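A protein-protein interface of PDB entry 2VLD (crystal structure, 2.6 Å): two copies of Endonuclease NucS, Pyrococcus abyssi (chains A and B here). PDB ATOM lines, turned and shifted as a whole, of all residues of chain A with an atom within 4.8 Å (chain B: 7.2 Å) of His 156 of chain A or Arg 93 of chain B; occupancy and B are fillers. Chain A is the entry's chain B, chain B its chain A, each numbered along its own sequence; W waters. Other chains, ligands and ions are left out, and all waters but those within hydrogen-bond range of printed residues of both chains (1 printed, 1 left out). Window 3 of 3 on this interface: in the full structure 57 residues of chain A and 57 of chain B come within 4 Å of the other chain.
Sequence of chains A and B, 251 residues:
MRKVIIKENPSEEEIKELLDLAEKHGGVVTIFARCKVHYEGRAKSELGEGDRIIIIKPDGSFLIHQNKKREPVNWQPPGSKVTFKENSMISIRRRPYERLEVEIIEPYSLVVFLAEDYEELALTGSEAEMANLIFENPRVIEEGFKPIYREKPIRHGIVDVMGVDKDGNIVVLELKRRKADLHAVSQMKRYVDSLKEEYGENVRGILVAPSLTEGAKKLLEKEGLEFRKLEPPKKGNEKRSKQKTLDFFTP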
ATOM      1  N   ILE A 154      -0.514 -18.048  37.202  1.00  0.00           N
ATOM      2  CA  ILE A 154       0.750 -18.603  36.769  1.00  0.00           C
ATOM      3  C   ILE A 154       1.120 -17.911  35.446  1.00  0.00           C
ATOM      4  O   ILE A 154       0.301 -17.174  34.898  1.00  0.00           O
ATOM      5  CB  ILE A 154       0.599 -20.152  36.688  1.00  0.00           C
ATOM      6  CG1 ILE A 154       1.439 -20.793  37.770  1.00  0.00           C
ATOM      7  CG2 ILE A 154       0.981 -20.744  35.352  1.00  0.00           C
ATOM      8  CD1 ILE A 154       1.087 -20.316  39.157  1.00  0.00           C
ATOM      9  N   ARG A 155       2.337 -18.100  34.944  1.00  0.00           N
ATOM     10  CA  ARG A 155       2.737 -17.444  33.691  1.00  0.00           C
ATOM     11  C   ARG A 155       1.764 -17.715  32.540  1.00  0.00           C
ATOM     12  O   ARG A 155       1.331 -16.781  31.853  1.00  0.00           O
ATOM     13  CB  ARG A 155       4.155 -17.827  33.277  1.00  0.00           C
ATOM     14  CG  ARG A 155       5.259 -17.036  33.961  1.00  0.00           C
ATOM     15  CD  ARG A 155       6.609 -17.526  33.461  1.00  0.00           C
ATOM     16  NE  ARG A 155       7.737 -16.995  34.224  1.00  0.00           N
ATOM     17  CZ  ARG A 155       9.015 -17.175  33.895  1.00  0.00           C
ATOM     18  NH1 ARG A 155       9.339 -17.873  32.812  1.00  0.00           N
ATOM     19  NH2 ARG A 155       9.974 -16.654  34.650  1.00  0.00           N
ATOM     20  N   HIS A 156       1.416 -18.987  32.341  1.00  0.00           N
ATOM     21  CA  HIS A 156       0.470 -19.371  31.285  1.00  0.00           C
ATOM     22  C   HIS A 156      -0.790 -20.021  31.830  1.00  0.00           C
ATOM     23  O   HIS A 156      -1.245 -21.027  31.292  1.00  0.00           O
ATOM     24  CB  HIS A 156       1.110 -20.334  30.273  1.00  0.00           C
ATOM     25  CG  HIS A 156       2.428 -19.877  29.739  1.00  0.00           C
ATOM     26  ND1 HIS A 156       2.647 -18.595  29.285  1.00  0.00           N
ATOM     27  CD2 HIS A 156       3.596 -20.543  29.567  1.00  0.00           C
ATOM     28  CE1 HIS A 156       3.897 -18.484  28.871  1.00  0.00           C
ATOM     29  NE2 HIS A 156       4.493 -19.652  29.029  1.00  0.00           N
ATOM     30  N   GLY A 157      -1.362 -19.462  32.885  1.00  0.00           N
ATOM     31  CA  GLY A 157      -2.640 -19.966  33.344  1.00  0.00           C
ATOM     32  C   GLY A 157      -2.928 -19.823  34.809  1.00  0.00           C
ATOM     33  O   GLY A 157      -2.282 -19.047  35.506  1.00  0.00           O
ATOM     34  N   ILE A 158      -3.914 -20.588  35.267  1.00  0.00           N
ATOM     35  CA  ILE A 158      -4.381 -20.503  36.639  1.00  0.00           C
ATOM     36  C   ILE A 158      -4.489 -21.882  37.235  1.00  0.00           C
ATOM     37  O   ILE A 158      -5.118 -22.772  36.661  1.00  0.00           O
ATOM     38  CB  ILE A 158      -5.712 -19.748  36.722  1.00  0.00           C
ATOM     39  CG1 ILE A 158      -5.529 -18.358  36.093  1.00  0.00           C
ATOM     40  CG2 ILE A 158      -6.210 -19.671  38.168  1.00  0.00           C
ATOM     41  CD1 ILE A 158      -6.614 -17.371  36.381  1.00  0.00           C
ATOM     42  N   ARG A 190      -0.079 -28.193  30.900  1.00  0.00           N
ATOM     43  CA  ARG A 190       0.305 -26.837  30.564  1.00  0.00           C
ATOM     44  C   ARG A 190       0.818 -26.103  31.799  1.00  0.00           C
ATOM     45  O   ARG A 190       1.879 -25.490  31.757  1.00  0.00           O
ATOM     46  CB  ARG A 190      -0.863 -26.090  29.924  1.00  0.00           C
ATOM     47  CG  ARG A 190      -0.441 -24.897  29.111  1.00  0.00           C
ATOM     48  CD  ARG A 190      -1.589 -24.311  28.330  1.00  0.00           C
ATOM     49  NE  ARG A 190      -2.399 -23.424  29.160  1.00  0.00           N
ATOM     50  CZ  ARG A 190      -3.657 -23.670  29.525  1.00  0.00           C
ATOM     51  NH1 ARG A 190      -4.262 -24.771  29.104  1.00  0.00           N
ATOM     52  NH2 ARG A 190      -4.306 -22.807  30.291  1.00  0.00           N
ATOM     53  N   TYR A 191       0.082 -26.201  32.906  1.00  0.00           N
ATOM     54  CA  TYR A 191       0.465 -25.528  34.154  1.00  0.00           C
ATOM     55  C   TYR A 191       1.797 -26.048  34.641  1.00  0.00           C
ATOM     56  O   TYR A 191       2.683 -25.273  34.978  1.00  0.00           O
ATOM     57  CB  TYR A 191      -0.599 -25.694  35.257  1.00  0.00           C
ATOM     58  CG  TYR A 191      -2.003 -25.306  34.856  1.00  0.00           C
ATOM     59  CD1 TYR A 191      -3.108 -26.048  35.306  1.00  0.00           C
ATOM     60  CD2 TYR A 191      -2.239 -24.202  34.026  1.00  0.00           C
ATOM     61  CE1 TYR A 191      -4.410 -25.701  34.944  1.00  0.00           C
ATOM     62  CE2 TYR A 191      -3.529 -23.850  33.661  1.00  0.00           C
ATOM     63  CZ  TYR A 191      -4.608 -24.608  34.123  1.00  0.00           C
ATOM     64  OH  TYR A 191      -5.877 -24.274  33.759  1.00  0.00           O
ATOM     65  N   SER A 194       4.689 -24.868  32.287  1.00  0.00           N
ATOM     66  CA  SER A 194       4.902 -23.451  32.592  1.00  0.00           C
ATOM     67  C   SER A 194       5.777 -23.267  33.836  1.00  0.00           C
ATOM     68  O   SER A 194       6.766 -22.518  33.812  1.00  0.00           O
ATOM     69  CB  SER A 194       3.557 -22.738  32.772  1.00  0.00           C
ATOM     70  OG  SER A 194       3.714 -21.439  33.320  1.00  0.00           O
ATOM     71  N   GLU B  40      -9.628 -18.744  31.416  1.00  0.00           N
ATOM     72  CA  GLU B  40      -8.682 -18.413  32.456  1.00  0.00           C
ATOM     73  C   GLU B  40      -8.301 -16.956  32.254  1.00  0.00           C
ATOM     74  O   GLU B  40      -7.731 -16.601  31.223  1.00  0.00           O
ATOM     75  CB  GLU B  40      -7.437 -19.277  32.338  1.00  0.00           C
ATOM     76  CG  GLU B  40      -7.642 -20.737  32.668  1.00  0.00           C
ATOM     77  CD  GLU B  40      -6.476 -21.609  32.211  1.00  0.00           C
ATOM     78  OE1 GLU B  40      -5.337 -21.099  32.077  1.00  0.00           O
ATOM     79  OE2 GLU B  40      -6.710 -22.815  31.973  1.00  0.00           O
ATOM     80  N   GLY B  79      -6.855  -7.701  19.230  1.00  0.00           N
ATOM     81  CA  GLY B  79      -5.444  -7.827  19.553  1.00  0.00           C
ATOM     82  C   GLY B  79      -5.094  -9.136  20.233  1.00  0.00           C
ATOM     83  O   GLY B  79      -3.946  -9.331  20.658  1.00  0.00           O
ATOM     84  N   SER B  80      -6.072 -10.027  20.330  1.00  0.00           N
ATOM     85  CA  SER B  80      -5.882 -11.349  20.908  1.00  0.00           C
ATOM     86  C   SER B  80      -5.574 -12.311  19.776  1.00  0.00           C
ATOM     87  O   SER B  80      -6.114 -12.173  18.686  1.00  0.00           O
ATOM     88  CB  SER B  80      -7.155 -11.809  21.633  1.00  0.00           C
ATOM     89  OG  SER B  80      -7.701 -10.813  22.475  1.00  0.00           O
ATOM     90  N   LYS B  81      -4.726 -13.297  20.044  1.00  0.00           N
ATOM     91  CA  LYS B  81      -4.188 -14.183  18.999  1.00  0.00           C
ATOM     92  C   LYS B  81      -4.943 -15.519  18.971  1.00  0.00           C
ATOM     93  O   LYS B  81      -5.274 -16.068  20.021  1.00  0.00           O
ATOM     94  CB  LYS B  81      -2.667 -14.353  19.192  1.00  0.00           C
ATOM     95  CG  LYS B  81      -1.971 -15.422  18.338  1.00  0.00           C
ATOM     96  CD  LYS B  81      -1.912 -15.074  16.851  1.00  0.00           C
ATOM     97  CE  LYS B  81      -1.469 -16.283  16.029  1.00  0.00           C
ATOM     98  NZ  LYS B  81      -1.490 -16.005  14.563  1.00  0.00           N
ATOM     99  N   THR B  83      -5.585 -19.597  17.703  1.00  0.00           N
ATOM    100  CA  THR B  83      -4.821 -20.830  17.597  1.00  0.00           C
ATOM    101  C   THR B  83      -5.774 -22.016  17.486  1.00  0.00           C
ATOM    102  O   THR B  83      -6.845 -21.986  18.080  1.00  0.00           O
ATOM    103  CB  THR B  83      -3.909 -20.964  18.838  1.00  0.00           C
ATOM    104  OG1 THR B  83      -2.643 -20.366  18.554  1.00  0.00           O
ATOM    105  CG2 THR B  83      -3.683 -22.405  19.242  1.00  0.00           C
ATOM    106  N   ILE B  90      -8.215 -18.248  22.051  1.00  0.00           N
ATOM    107  CA  ILE B  90      -7.789 -16.876  21.895  1.00  0.00           C
ATOM    108  C   ILE B  90      -7.108 -16.465  23.189  1.00  0.00           C
ATOM    109  O   ILE B  90      -7.709 -16.520  24.269  1.00  0.00           O
ATOM    110  CB  ILE B  90      -8.955 -15.941  21.399  1.00  0.00           C
ATOM    111  CG1 ILE B  90      -8.434 -14.553  21.029  1.00  0.00           C
ATOM    112  CG2 ILE B  90     -10.035 -15.808  22.402  1.00  0.00           C
ATOM    113  CD1 ILE B  90      -8.963 -14.027  19.653  1.00  0.00           C
ATOM    114  N   SER B  91      -5.826 -16.136  23.074  1.00  0.00           N
ATOM    115  CA  SER B  91      -5.031 -15.716  24.210  1.00  0.00           C
ATOM    116  C   SER B  91      -4.653 -14.262  24.051  1.00  0.00           C
ATOM    117  O   SER B  91      -4.158 -13.840  23.001  1.00  0.00           O
ATOM    118  CB  SER B  91      -3.749 -16.549  24.352  1.00  0.00           C
ATOM    119  OG  SER B  91      -4.028 -17.930  24.308  1.00  0.00           O
ATOM    120  N   ILE B  92      -4.904 -13.497  25.101  1.00  0.00           N
ATOM    121  CA  ILE B  92      -4.331 -12.180  25.234  1.00  0.00           C
ATOM    122  C   ILE B  92      -3.304 -12.307  26.361  1.00  0.00           C
ATOM    123  O   ILE B  92      -3.641 -12.427  27.530  1.00  0.00           O
ATOM    124  CB  ILE B  92      -5.433 -11.018  25.373  1.00  0.00           C
ATOM    125  CG1 ILE B  92      -4.807  -9.617  25.263  1.00  0.00           C
ATOM    126  CG2 ILE B  92      -6.284 -11.139  26.637  1.00  0.00           C
ATOM    127  CD1 ILE B  92      -5.709  -8.503  24.652  1.00  0.00           C
ATOM    128  N   ARG B  93      -2.037 -12.385  25.995  1.00  0.00           N
ATOM    129  CA  ARG B  93      -1.000 -12.180  26.994  1.00  0.00           C
ATOM    130  C   ARG B  93      -0.557 -10.744  26.902  1.00  0.00           C
ATOM    131  O   ARG B  93       0.631 -10.437  27.054  1.00  0.00           O
ATOM    132  CB  ARG B  93       0.181 -13.142  26.855  1.00  0.00           C
ATOM    133  CG  ARG B  93       0.440 -13.694  25.479  1.00  0.00           C
ATOM    134  CD  ARG B  93       1.346 -14.864  25.673  1.00  0.00           C
ATOM    135  NE  ARG B  93       1.054 -16.011  24.827  1.00  0.00           N
ATOM    136  CZ  ARG B  93       1.135 -17.270  25.249  1.00  0.00           C
ATOM    137  NH1 ARG B  93       1.469 -17.530  26.511  1.00  0.00           N
ATOM    138  NH2 ARG B  93       0.865 -18.271  24.423  1.00  0.00           N
ATOM    139  N   ARG B  94      -1.527  -9.868  26.639  1.00  0.00           N
ATOM    140  CA  ARG B  94      -1.262  -8.439  26.559  1.00  0.00           C
ATOM    141  C   ARG B  94      -1.403  -7.774  27.937  1.00  0.00           C
ATOM    142  O   ARG B  94      -2.124  -6.789  28.131  1.00  0.00           O
ATOM    143  CB  ARG B  94      -2.085  -7.762  25.456  1.00  0.00           C
ATOM    144  CG  ARG B  94      -1.610  -8.093  24.042  1.00  0.00           C
ATOM    145  CD  ARG B  94      -1.756  -6.872  23.130  1.00  0.00           C
ATOM    146  NE  ARG B  94      -1.368  -7.145  21.744  1.00  0.00           N
ATOM    147  CZ  ARG B  94      -1.676  -6.373  20.701  1.00  0.00           C
ATOM    148  NH1 ARG B  94      -2.389  -5.260  20.861  1.00  0.00           N
ATOM    149  NH2 ARG B  94      -1.275  -6.723  19.483  1.00  0.00           N
ATOM    150  N   ARG B  95      -0.701  -8.391  28.886  1.00  0.00           N
ATOM    151  CA  ARG B  95      -0.298  -7.810  30.171  1.00  0.00           C
ATOM    152  C   ARG B  95      -1.200  -7.997  31.396  1.00  0.00           C
ATOM    153  O   ARG B  95      -0.739  -7.795  32.538  1.00  0.00           O
ATOM    154  CB  ARG B  95       0.329  -6.408  30.057  1.00  0.00           C
ATOM    155  CG  ARG B  95       1.852  -6.475  30.165  1.00  0.00           C
ATOM    156  CD  ARG B  95       2.254  -7.549  31.183  1.00  0.00           C
ATOM    157  NE  ARG B  95       3.676  -7.589  31.511  1.00  0.00           N
ATOM    158  CZ  ARG B  95       4.293  -8.660  32.010  1.00  0.00           C
ATOM    159  NH1 ARG B  95       3.621  -9.791  32.216  1.00  0.00           N
ATOM    160  NH2 ARG B  95       5.587  -8.611  32.291  1.00  0.00           N
ATOM    161  N   PRO B  96      -2.487  -8.299  31.174  1.00  0.00           N
ATOM    162  CA  PRO B  96      -2.985  -9.447  31.902  1.00  0.00           C
ATOM    163  C   PRO B  96      -2.791 -10.658  30.986  1.00  0.00           C
ATOM    164  O   PRO B  96      -2.528 -10.485  29.791  1.00  0.00           O
ATOM    165  CB  PRO B  96      -4.474  -9.128  32.101  1.00  0.00           C
ATOM    166  CG  PRO B  96      -4.712  -7.782  31.423  1.00  0.00           C
ATOM    167  CD  PRO B  96      -3.570  -7.591  30.479  1.00  0.00           C
ATOM    168  N   TYR B  97      -2.871 -11.863  31.541  1.00  0.00           N
ATOM    169  CA  TYR B  97      -2.918 -13.073  30.737  1.00  0.00           C
ATOM    170  C   TYR B  97      -4.352 -13.551  30.718  1.00  0.00           C
ATOM    171  O   TYR B  97      -5.002 -13.604  31.756  1.00  0.00           O
ATOM    172  CB  TYR B  97      -2.005 -14.167  31.304  1.00  0.00           C
ATOM    173  CG  TYR B  97      -2.245 -15.537  30.699  1.00  0.00           C
ATOM    174  CD1 TYR B  97      -1.699 -15.878  29.462  1.00  0.00           C
ATOM    175  CD2 TYR B  97      -3.029 -16.492  31.361  1.00  0.00           C
ATOM    176  CE1 TYR B  97      -1.917 -17.142  28.891  1.00  0.00           C
ATOM    177  CE2 TYR B  97      -3.268 -17.757  30.795  1.00  0.00           C
ATOM    178  CZ  TYR B  97      -2.710 -18.076  29.563  1.00  0.00           C
ATOM    179  OH  TYR B  97      -2.928 -19.321  29.003  1.00  0.00           O
ATOM    180  N   GLU B  98      -4.848 -13.899  29.537  1.00  0.00           N
ATOM    181  CA  GLU B  98      -6.206 -14.392  29.401  1.00  0.00           C
ATOM    182  C   GLU B  98      -6.309 -15.467  28.343  1.00  0.00           C
ATOM    183  O   GLU B  98      -5.800 -15.301  27.236  1.00  0.00           O
ATOM    184  CB  GLU B  98      -7.151 -13.254  29.043  1.00  0.00           C
ATOM    185  CG  GLU B  98      -7.405 -12.261  30.163  1.00  0.00           C
ATOM    186  CD  GLU B  98      -8.448 -11.236  29.780  1.00  0.00           C
ATOM    187  OE1 GLU B  98      -9.637 -11.606  29.693  1.00  0.00           O
ATOM    188  OE2 GLU B  98      -8.072 -10.064  29.561  1.00  0.00           O
ATOM    189  N   ARG B  99      -6.991 -16.560  28.684  1.00  0.00           N
ATOM    190  CA  ARG B  99      -7.173 -17.667  27.757  1.00  0.00           C
ATOM    191  C   ARG B  99      -8.633 -18.043  27.611  1.00  0.00           C
ATOM    192  O   ARG B  99      -9.273 -18.446  28.574  1.00  0.00           O
ATOM    193  CB  ARG B  99      -6.377 -18.901  28.207  1.00  0.00           C
ATOM    194  CG  ARG B  99      -5.911 -19.776  27.051  1.00  0.00           C
ATOM    195  CD  ARG B  99      -5.161 -21.012  27.529  1.00  0.00           C
ATOM    196  NE  ARG B  99      -6.065 -22.153  27.578  1.00  0.00           N
ATOM    197  CZ  ARG B  99      -6.012 -23.186  26.748  1.00  0.00           C
ATOM    198  NH1 ARG B  99      -5.078 -23.250  25.814  1.00  0.00           N
ATOM    199  NH2 ARG B  99      -6.890 -24.166  26.860  1.00  0.00           N
HETATM  200  O   HOH W   1      -2.503 -22.390  25.892  1.00  0.00           O
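OG of Ser 194 of chain A sits close to N of His 156 of chain A (3.5 Å).
The side-chain hydroxyl (OH) of Tyr 191 of chain A lies close to the backbone carbonyl oxygen (O) of Ile 158 of chain A, 3.4 Å away.
The backbone NH of Arg 99 of chain B is in hydrogen-bond range of the backbone carbonyl oxygen of Glu 40 of chain B, 2.6 Å away.
The backbone carbonyl oxygen of His 156 of chain A sits at hydrogen-bond distance from the guanidinium group of Arg 190 of chain A (3.4 Å).
Of the 8 printed residues of chain A, 6 touch a printed residue of chain B.
Printed residues of chain B that touch a printed residue of chain A: Glu 40, Arg 93, Tyr 97 and Arg 99.
Among the printed residues, Asp or Glu carboxylates within 4 Å of a Lys or Arg side-chain nitrogen of the other chain: Arg 190 of chain A with Glu 40 of chain B (2.7 Å).
Printed residues of chain B within 4 Å of Arg 155 of chain A: Tyr 97 (3.96 Å).
His 156 of chain A touches just these residues of chain B: Arg 93 and Tyr 97.
Arg 93 of chain B touches one residue of chain A.
Printed residues of chain A within 4 Å of Arg 99 of chain B: Arg 190 (3.3 Å).
The nearest residue of chain B that does not touch His 156 of chain A is Glu 40 of chain B (4.2 Å).
No position is printed for both chains.
Of the 10 pairs that touch across the chains among the printed residues, none has its exchanged pair printed and touching as well.
Water W1 bridges NH1 of Arg 99 of chain B (2.7 Å) and NE of Arg 190 of chain A (3.4 Å).
OH of Tyr 97 of chain B is in hydrogen-bond range of O of His 156 of chain A (3.3 Å).
NH1 of Arg 93 of chain B sits at hydrogen-bond distance from ND1 of His 156 of chain A, at 3.2 Å.
OE2 of Glu 40 of chain B sits at hydrogen-bond distance from OH of Tyr 191 of chain A, 2.5 Å away.
The side-chain carboxylate of Glu 40 of chain B lies within salt-bridge range of the guanidinium group of Arg 190 of chain A (2.7 Å).
NH2 of Arg 190 of chain A lies close to NE of Arg 99 of chain B, at 3.3 Å.
Among the printed residues, merely in contact across the chains: Gly 157 of chain A with Glu 40 of chain B (3.2 Å), Gly 157 of chain A with Tyr 97 of chain B (3.3 Å), Ile 158 of chain A with Glu 40 of chain B (3.5 Å), Arg 155 of chain A with Tyr 97 of chain B (3.96 Å) and Arg 190 of chain A with Tyr 97 of chain B (3.96 Å).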
